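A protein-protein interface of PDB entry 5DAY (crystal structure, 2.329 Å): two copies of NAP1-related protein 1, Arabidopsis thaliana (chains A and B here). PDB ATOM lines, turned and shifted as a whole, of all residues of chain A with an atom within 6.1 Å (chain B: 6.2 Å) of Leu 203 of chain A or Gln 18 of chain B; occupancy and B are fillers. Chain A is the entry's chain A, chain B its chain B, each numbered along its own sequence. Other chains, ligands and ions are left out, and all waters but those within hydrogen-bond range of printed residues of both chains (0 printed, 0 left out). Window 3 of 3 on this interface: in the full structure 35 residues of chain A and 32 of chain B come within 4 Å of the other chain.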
ATOM      1  N   PHE A  63     -31.306 -31.686 -11.716  1.00  0.00           N
ATOM      2  CA  PHE A  63     -30.588 -30.825 -12.654  1.00  0.00           C
ATOM      3  C   PHE A  63     -29.562 -31.591 -13.477  1.00  0.00           C
ATOM      4  O   PHE A  63     -29.660 -31.654 -14.705  1.00  0.00           O
ATOM      5  CB  PHE A  63     -29.897 -29.665 -11.934  1.00  0.00           C
ATOM      6  CG  PHE A  63     -29.164 -28.743 -12.877  1.00  0.00           C
ATOM      7  CD1 PHE A  63     -29.844 -27.748 -13.574  1.00  0.00           C
ATOM      8  CD2 PHE A  63     -27.792 -28.893 -13.097  1.00  0.00           C
ATOM      9  CE1 PHE A  63     -29.150 -26.897 -14.464  1.00  0.00           C
ATOM     10  CE2 PHE A  63     -27.101 -28.048 -13.984  1.00  0.00           C
ATOM     11  CZ  PHE A  63     -27.771 -27.060 -14.663  1.00  0.00           C
ATOM     12  N   ALA A  67     -29.597 -32.216 -17.444  1.00  0.00           N
ATOM     13  CA  ALA A  67     -28.672 -31.607 -18.396  1.00  0.00           C
ATOM     14  C   ALA A  67     -27.898 -32.676 -19.160  1.00  0.00           C
ATOM     15  O   ALA A  67     -27.674 -32.550 -20.368  1.00  0.00           O
ATOM     16  CB  ALA A  67     -27.712 -30.662 -17.667  1.00  0.00           C
ATOM     17  N   LEU A 198     -20.659 -29.931 -20.961  1.00  0.00           N
ATOM     18  CA  LEU A 198     -21.623 -30.042 -19.880  1.00  0.00           C
ATOM     19  C   LEU A 198     -21.147 -29.336 -18.615  1.00  0.00           C
ATOM     20  O   LEU A 198     -21.933 -28.659 -17.941  1.00  0.00           O
ATOM     21  CB  LEU A 198     -21.875 -31.520 -19.602  1.00  0.00           C
ATOM     22  CG  LEU A 198     -23.030 -31.785 -18.663  1.00  0.00           C
ATOM     23  CD1 LEU A 198     -24.352 -31.609 -19.409  1.00  0.00           C
ATOM     24  CD2 LEU A 198     -22.886 -33.185 -18.084  1.00  0.00           C
ATOM     25  N   ASN A 201     -21.020 -25.170 -19.216  1.00  0.00           N
ATOM     26  CA  ASN A 201     -22.339 -24.562 -19.096  1.00  0.00           C
ATOM     27  C   ASN A 201     -23.400 -25.640 -19.239  1.00  0.00           C
ATOM     28  O   ASN A 201     -23.933 -25.871 -20.330  1.00  0.00           O
ATOM     29  CB  ASN A 201     -22.550 -23.450 -20.126  1.00  0.00           C
ATOM     30  CG  ASN A 201     -23.799 -22.635 -19.834  1.00  0.00           C
ATOM     31  OD1 ASN A 201     -24.706 -23.094 -19.137  1.00  0.00           O
ATOM     32  ND2 ASN A 201     -23.840 -21.420 -20.334  1.00  0.00           N
ATOM     33  N   PRO A 202     -23.756 -26.311 -18.140  1.00  0.00           N
ATOM     34  CA  PRO A 202     -24.850 -27.286 -18.210  1.00  0.00           C
ATOM     35  C   PRO A 202     -26.187 -26.629 -18.433  1.00  0.00           C
ATOM     36  O   PRO A 202     -27.136 -27.310 -18.838  1.00  0.00           O
ATOM     37  CB  PRO A 202     -24.804 -27.961 -16.837  1.00  0.00           C
ATOM     38  CG  PRO A 202     -24.324 -26.855 -15.924  1.00  0.00           C
ATOM     39  CD  PRO A 202     -23.281 -26.103 -16.760  1.00  0.00           C
ATOM     40  N   LEU A 203     -26.290 -25.327 -18.169  1.00  0.00           N
ATOM     41  CA  LEU A 203     -27.581 -24.664 -18.238  1.00  0.00           C
ATOM     42  C   LEU A 203     -28.079 -24.580 -19.670  1.00  0.00           C
ATOM     43  O   LEU A 203     -29.292 -24.655 -19.893  1.00  0.00           O
ATOM     44  CB  LEU A 203     -27.502 -23.276 -17.599  1.00  0.00           C
ATOM     45  CG  LEU A 203     -28.786 -22.460 -17.602  1.00  0.00           C
ATOM     46  CD1 LEU A 203     -29.842 -23.184 -16.808  1.00  0.00           C
ATOM     47  CD2 LEU A 203     -28.577 -21.071 -17.064  1.00  0.00           C
ATOM     48  N   THR A 204     -27.172 -24.472 -20.656  1.00  0.00           N
ATOM     49  CA  THR A 204     -27.644 -24.397 -22.033  1.00  0.00           C
ATOM     50  C   THR A 204     -28.166 -25.735 -22.521  1.00  0.00           C
ATOM     51  O   THR A 204     -28.877 -25.780 -23.527  1.00  0.00           O
ATOM     52  CB  THR A 204     -26.558 -23.863 -23.004  1.00  0.00           C
ATOM     53  OG1 THR A 204     -25.378 -24.668 -22.963  1.00  0.00           O
ATOM     54  CG2 THR A 204     -26.198 -22.405 -22.677  1.00  0.00           C
ATOM     55  N   TYR A 205     -27.853 -26.824 -21.834  1.00  0.00           N
ATOM     56  CA  TYR A 205     -28.552 -28.061 -22.155  1.00  0.00           C
ATOM     57  C   TYR A 205     -29.782 -28.246 -21.296  1.00  0.00           C
ATOM     58  O   TYR A 205     -30.754 -28.861 -21.744  1.00  0.00           O
ATOM     59  CB  TYR A 205     -27.595 -29.255 -22.051  1.00  0.00           C
ATOM     60  CG  TYR A 205     -26.348 -28.985 -22.893  1.00  0.00           C
ATOM     61  CD1 TYR A 205     -26.368 -29.130 -24.281  1.00  0.00           C
ATOM     62  CD2 TYR A 205     -25.179 -28.518 -22.303  1.00  0.00           C
ATOM     63  CE1 TYR A 205     -25.241 -28.854 -25.049  1.00  0.00           C
ATOM     64  CE2 TYR A 205     -24.051 -28.245 -23.055  1.00  0.00           C
ATOM     65  CZ  TYR A 205     -24.093 -28.407 -24.423  1.00  0.00           C
ATOM     66  OH  TYR A 205     -22.969 -28.128 -25.145  1.00  0.00           O
ATOM     67  N   PHE A 206     -29.785 -27.681 -20.091  1.00  0.00           N
ATOM     68  CA  PHE A 206     -30.955 -27.792 -19.233  1.00  0.00           C
ATOM     69  C   PHE A 206     -32.119 -26.977 -19.789  1.00  0.00           C
ATOM     70  O   PHE A 206     -33.272 -27.422 -19.710  1.00  0.00           O
ATOM     71  CB  PHE A 206     -30.611 -27.358 -17.809  1.00  0.00           C
ATOM     72  CG  PHE A 206     -31.763 -27.485 -16.846  1.00  0.00           C
ATOM     73  CD1 PHE A 206     -31.997 -28.681 -16.181  1.00  0.00           C
ATOM     74  CD2 PHE A 206     -32.615 -26.420 -16.614  1.00  0.00           C
ATOM     75  CE1 PHE A 206     -33.044 -28.817 -15.308  1.00  0.00           C
ATOM     76  CE2 PHE A 206     -33.686 -26.547 -15.735  1.00  0.00           C
ATOM     77  CZ  PHE A 206     -33.895 -27.748 -15.077  1.00  0.00           C
ATOM     78  N   ASN A 207     -31.827 -25.806 -20.373  1.00  0.00           N
ATOM     79  CA  ASN A 207     -32.825 -24.888 -20.957  1.00  0.00           C
ATOM     80  C   ASN A 207     -33.331 -25.273 -22.357  1.00  0.00           C
ATOM     81  O   ASN A 207     -32.986 -26.322 -22.885  1.00  0.00           O
ATOM     82  CB  ASN A 207     -32.251 -23.474 -21.032  1.00  0.00           C
ATOM     83  CG  ASN A 207     -32.179 -22.813 -19.692  1.00  0.00           C
ATOM     84  OD1 ASN A 207     -32.817 -23.250 -18.742  1.00  0.00           O
ATOM     85  ND2 ASN A 207     -31.407 -21.741 -19.600  1.00  0.00           N
ATOM     86  N   SER B  13     -33.954 -20.202  -8.971  1.00  0.00           N
ATOM     87  CA  SER B  13     -32.707 -20.952  -9.063  1.00  0.00           C
ATOM     88  C   SER B  13     -32.140 -20.905 -10.471  1.00  0.00           C
ATOM     89  O   SER B  13     -30.924 -20.798 -10.654  1.00  0.00           O
ATOM     90  CB  SER B  13     -32.930 -22.405  -8.652  1.00  0.00           C
ATOM     91  OG  SER B  13     -33.299 -22.465  -7.295  1.00  0.00           O
ATOM     92  N   ILE B  14     -33.008 -21.035 -11.471  1.00  0.00           N
ATOM     93  CA  ILE B  14     -32.602 -20.852 -12.858  1.00  0.00           C
ATOM     94  C   ILE B  14     -32.050 -19.446 -13.075  1.00  0.00           C
ATOM     95  O   ILE B  14     -30.986 -19.277 -13.682  1.00  0.00           O
ATOM     96  CB  ILE B  14     -33.777 -21.170 -13.797  1.00  0.00           C
ATOM     97  CG1 ILE B  14     -34.079 -22.663 -13.713  1.00  0.00           C
ATOM     98  CG2 ILE B  14     -33.433 -20.846 -15.233  1.00  0.00           C
ATOM     99  CD1 ILE B  14     -32.896 -23.501 -14.205  1.00  0.00           C
ATOM    100  N   GLU B  15     -32.744 -18.415 -12.579  1.00  0.00           N
ATOM    101  CA  GLU B  15     -32.209 -17.062 -12.759  1.00  0.00           C
ATOM    102  C   GLU B  15     -30.819 -16.947 -12.163  1.00  0.00           C
ATOM    103  O   GLU B  15     -29.920 -16.364 -12.775  1.00  0.00           O
ATOM    104  CB  GLU B  15     -33.105 -15.992 -12.130  1.00  0.00           C
ATOM    105  CG  GLU B  15     -34.424 -15.817 -12.788  1.00  0.00           C
ATOM    106  CD  GLU B  15     -34.306 -15.389 -14.229  1.00  0.00           C
ATOM    107  OE1 GLU B  15     -33.787 -14.269 -14.485  1.00  0.00           O
ATOM    108  OE2 GLU B  15     -34.745 -16.183 -15.098  1.00  0.00           O
ATOM    109  N   LYS B  16     -30.619 -17.507 -10.975  1.00  0.00           N
ATOM    110  CA  LYS B  16     -29.308 -17.410 -10.353  1.00  0.00           C
ATOM    111  C   LYS B  16     -28.281 -18.236 -11.108  1.00  0.00           C
ATOM    112  O   LYS B  16     -27.130 -17.825 -11.218  1.00  0.00           O
ATOM    113  CB  LYS B  16     -29.389 -17.831  -8.878  1.00  0.00           C
ATOM    114  CG  LYS B  16     -30.258 -16.860  -8.099  1.00  0.00           C
ATOM    115  CD  LYS B  16     -30.006 -16.854  -6.630  1.00  0.00           C
ATOM    116  CE  LYS B  16     -30.593 -18.031  -5.961  1.00  0.00           C
ATOM    117  NZ  LYS B  16     -30.673 -17.712  -4.483  1.00  0.00           N
ATOM    118  N   LEU B  17     -28.671 -19.401 -11.638  1.00  0.00           N
ATOM    119  CA  LEU B  17     -27.744 -20.159 -12.481  1.00  0.00           C
ATOM    120  C   LEU B  17     -27.345 -19.361 -13.707  1.00  0.00           C
ATOM    121  O   LEU B  17     -26.166 -19.346 -14.090  1.00  0.00           O
ATOM    122  CB  LEU B  17     -28.341 -21.488 -12.938  1.00  0.00           C
ATOM    123  CG  LEU B  17     -28.350 -22.619 -11.928  1.00  0.00           C
ATOM    124  CD1 LEU B  17     -28.836 -23.909 -12.616  1.00  0.00           C
ATOM    125  CD2 LEU B  17     -26.961 -22.790 -11.315  1.00  0.00           C
ATOM    126  N   GLN B  18     -28.312 -18.692 -14.341  1.00  0.00           N
ATOM    127  CA  GLN B  18     -27.996 -17.915 -15.533  1.00  0.00           C
ATOM    128  C   GLN B  18     -26.994 -16.816 -15.210  1.00  0.00           C
ATOM    129  O   GLN B  18     -26.093 -16.523 -16.005  1.00  0.00           O
ATOM    130  CB  GLN B  18     -29.270 -17.323 -16.140  1.00  0.00           C
ATOM    131  CG  GLN B  18     -29.011 -16.511 -17.383  1.00  0.00           C
ATOM    132  CD  GLN B  18     -28.384 -17.343 -18.511  1.00  0.00           C
ATOM    133  OE1 GLN B  18     -29.023 -18.264 -19.048  1.00  0.00           O
ATOM    134  NE2 GLN B  18     -27.130 -17.029 -18.867  1.00  0.00           N
ATOM    135  N   GLU B  19     -27.139 -16.208 -14.045  1.00  0.00           N
ATOM    136  CA  GLU B  19     -26.251 -15.135 -13.644  1.00  0.00           C
ATOM    137  C   GLU B  19     -24.863 -15.665 -13.319  1.00  0.00           C
ATOM    138  O   GLU B  19     -23.855 -14.998 -13.575  1.00  0.00           O
ATOM    139  CB  GLU B  19     -26.849 -14.424 -12.434  1.00  0.00           C
ATOM    140  CG  GLU B  19     -26.055 -13.221 -12.014  1.00  0.00           C
ATOM    141  CD  GLU B  19     -26.643 -12.554 -10.805  1.00  0.00           C
ATOM    142  OE1 GLU B  19     -27.772 -12.961 -10.398  1.00  0.00           O
ATOM    143  OE2 GLU B  19     -25.965 -11.635 -10.266  1.00  0.00           O
ATOM    144  N   ILE B  20     -24.791 -16.850 -12.723  1.00  0.00           N
ATOM    145  CA  ILE B  20     -23.498 -17.458 -12.460  1.00  0.00           C
ATOM    146  C   ILE B  20     -22.797 -17.805 -13.766  1.00  0.00           C
ATOM    147  O   ILE B  20     -21.587 -17.599 -13.901  1.00  0.00           O
ATOM    148  CB  ILE B  20     -23.673 -18.684 -11.553  1.00  0.00           C
ATOM    149  CG1 ILE B  20     -24.104 -18.218 -10.158  1.00  0.00           C
ATOM    150  CG2 ILE B  20     -22.401 -19.508 -11.529  1.00  0.00           C
ATOM    151  CD1 ILE B  20     -24.461 -19.313  -9.251  1.00  0.00           C
ATOM    152  N   GLN B  21     -23.540 -18.326 -14.747  1.00  0.00           N
ATOM    153  CA  GLN B  21     -22.938 -18.628 -16.045  1.00  0.00           C
ATOM    154  C   GLN B  21     -22.445 -17.360 -16.740  1.00  0.00           C
ATOM    155  O   GLN B  21     -21.415 -17.390 -17.427  1.00  0.00           O
ATOM    156  CB  GLN B  21     -23.917 -19.365 -16.965  1.00  0.00           C
ATOM    157  CG  GLN B  21     -24.244 -20.797 -16.577  1.00  0.00           C
ATOM    158  CD  GLN B  21     -23.025 -21.682 -16.353  1.00  0.00           C
ATOM    159  OE1 GLN B  21     -23.035 -22.531 -15.455  1.00  0.00           O
ATOM    160  NE2 GLN B  21     -21.985 -21.511 -17.172  1.00  0.00           N
ATOM    161  N   ASP B  22     -23.174 -16.246 -16.597  1.00  0.00           N
ATOM    162  CA  ASP B  22     -22.665 -14.978 -17.107  1.00  0.00           C
ATOM    163  C   ASP B  22     -21.356 -14.597 -16.420  1.00  0.00           C
ATOM    164  O   ASP B  22     -20.410 -14.169 -17.086  1.00  0.00           O
ATOM    165  CB  ASP B  22     -23.700 -13.858 -16.938  1.00  0.00           C
ATOM    166  CG  ASP B  22     -24.940 -14.043 -17.823  1.00  0.00           C
ATOM    167  OD1 ASP B  22     -24.872 -14.802 -18.819  1.00  0.00           O
ATOM    168  OD2 ASP B  22     -25.994 -13.427 -17.521  1.00  0.00           O
ATOM    169  N   ASP B  23     -21.273 -14.754 -15.093  1.00  0.00           N
ATOM    170  CA  ASP B  23     -20.020 -14.469 -14.393  1.00  0.00           C
ATOM    171  C   ASP B  23     -18.887 -15.348 -14.909  1.00  0.00           C
ATOM    172  O   ASP B  23     -17.767 -14.867 -15.105  1.00  0.00           O
ATOM    173  CB  ASP B  23     -20.167 -14.663 -12.880  1.00  0.00           C
ATOM    174  CG  ASP B  23     -21.035 -13.604 -12.234  1.00  0.00           C
ATOM    175  OD1 ASP B  23     -21.232 -12.534 -12.846  1.00  0.00           O
ATOM    176  OD2 ASP B  23     -21.541 -13.842 -11.109  1.00  0.00           O
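Hydrophobic or aromatic side chains of chain A within 4 Å of the printed part of chain B: Phe 63, Pro 202, Leu 203 and Phe 206. Of the 11 printed residues of chain B, 4 touch a printed residue of chain A. Among the printed residues, no Asp or Glu carboxylate lies within 4 Å of a Lys or Arg side-chain nitrogen of the other chain.
Printed residues of chain B within 4 Å of Asn 201 of chain A: Gln 21 (3.4 Å). Leu 203 of chain A touches just these residues of chain B: Leu 17 and Gln 18. Tyr 205 of chain A touches none of the printed residues of chain B. Printed residues of chain A within 4 Å of Ile 14 of chain B: Phe 206. Of the printed residues of chain A, Leu 17 of chain B touches Phe 63 (3.5 Å) and Leu 203 (3.96 Å). Of chain A, only Leu 203 (3.5 Å) comes within 4 Å of Gln 18 of chain B. The nearest residue of chain A that does not touch Gln 18 of chain B is Asn 207 of chain A (4.3 Å).
Among the printed residues, pairs that only touch across the chains: Asn 201 of chain A with Gln 21 of chain B, Leu 203 of chain A with Gln 18 of chain B, Phe 206 of chain A with Ile 14 of chain B, Phe 63 of chain A with Leu 17 of chain B, Pro 202 of chain A with Gln 21 of chain B and Leu 203 of chain A with Leu 17 of chain B.
No position is printed for both chains.
OD1 of Asn 201 of chain A is in hydrogen-bond range of N of Leu 203 of chain A (2.9 Å). N of Thr 204 of chain A sits at hydrogen-bond distance from OD1 of Asn 201 of chain A (3.2 Å). The side-chain amide nitrogen of Gln 18 of chain B is in hydrogen-bond range of the side-chain carboxylate of Asp 22 of chain B, at 3.2 Å.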
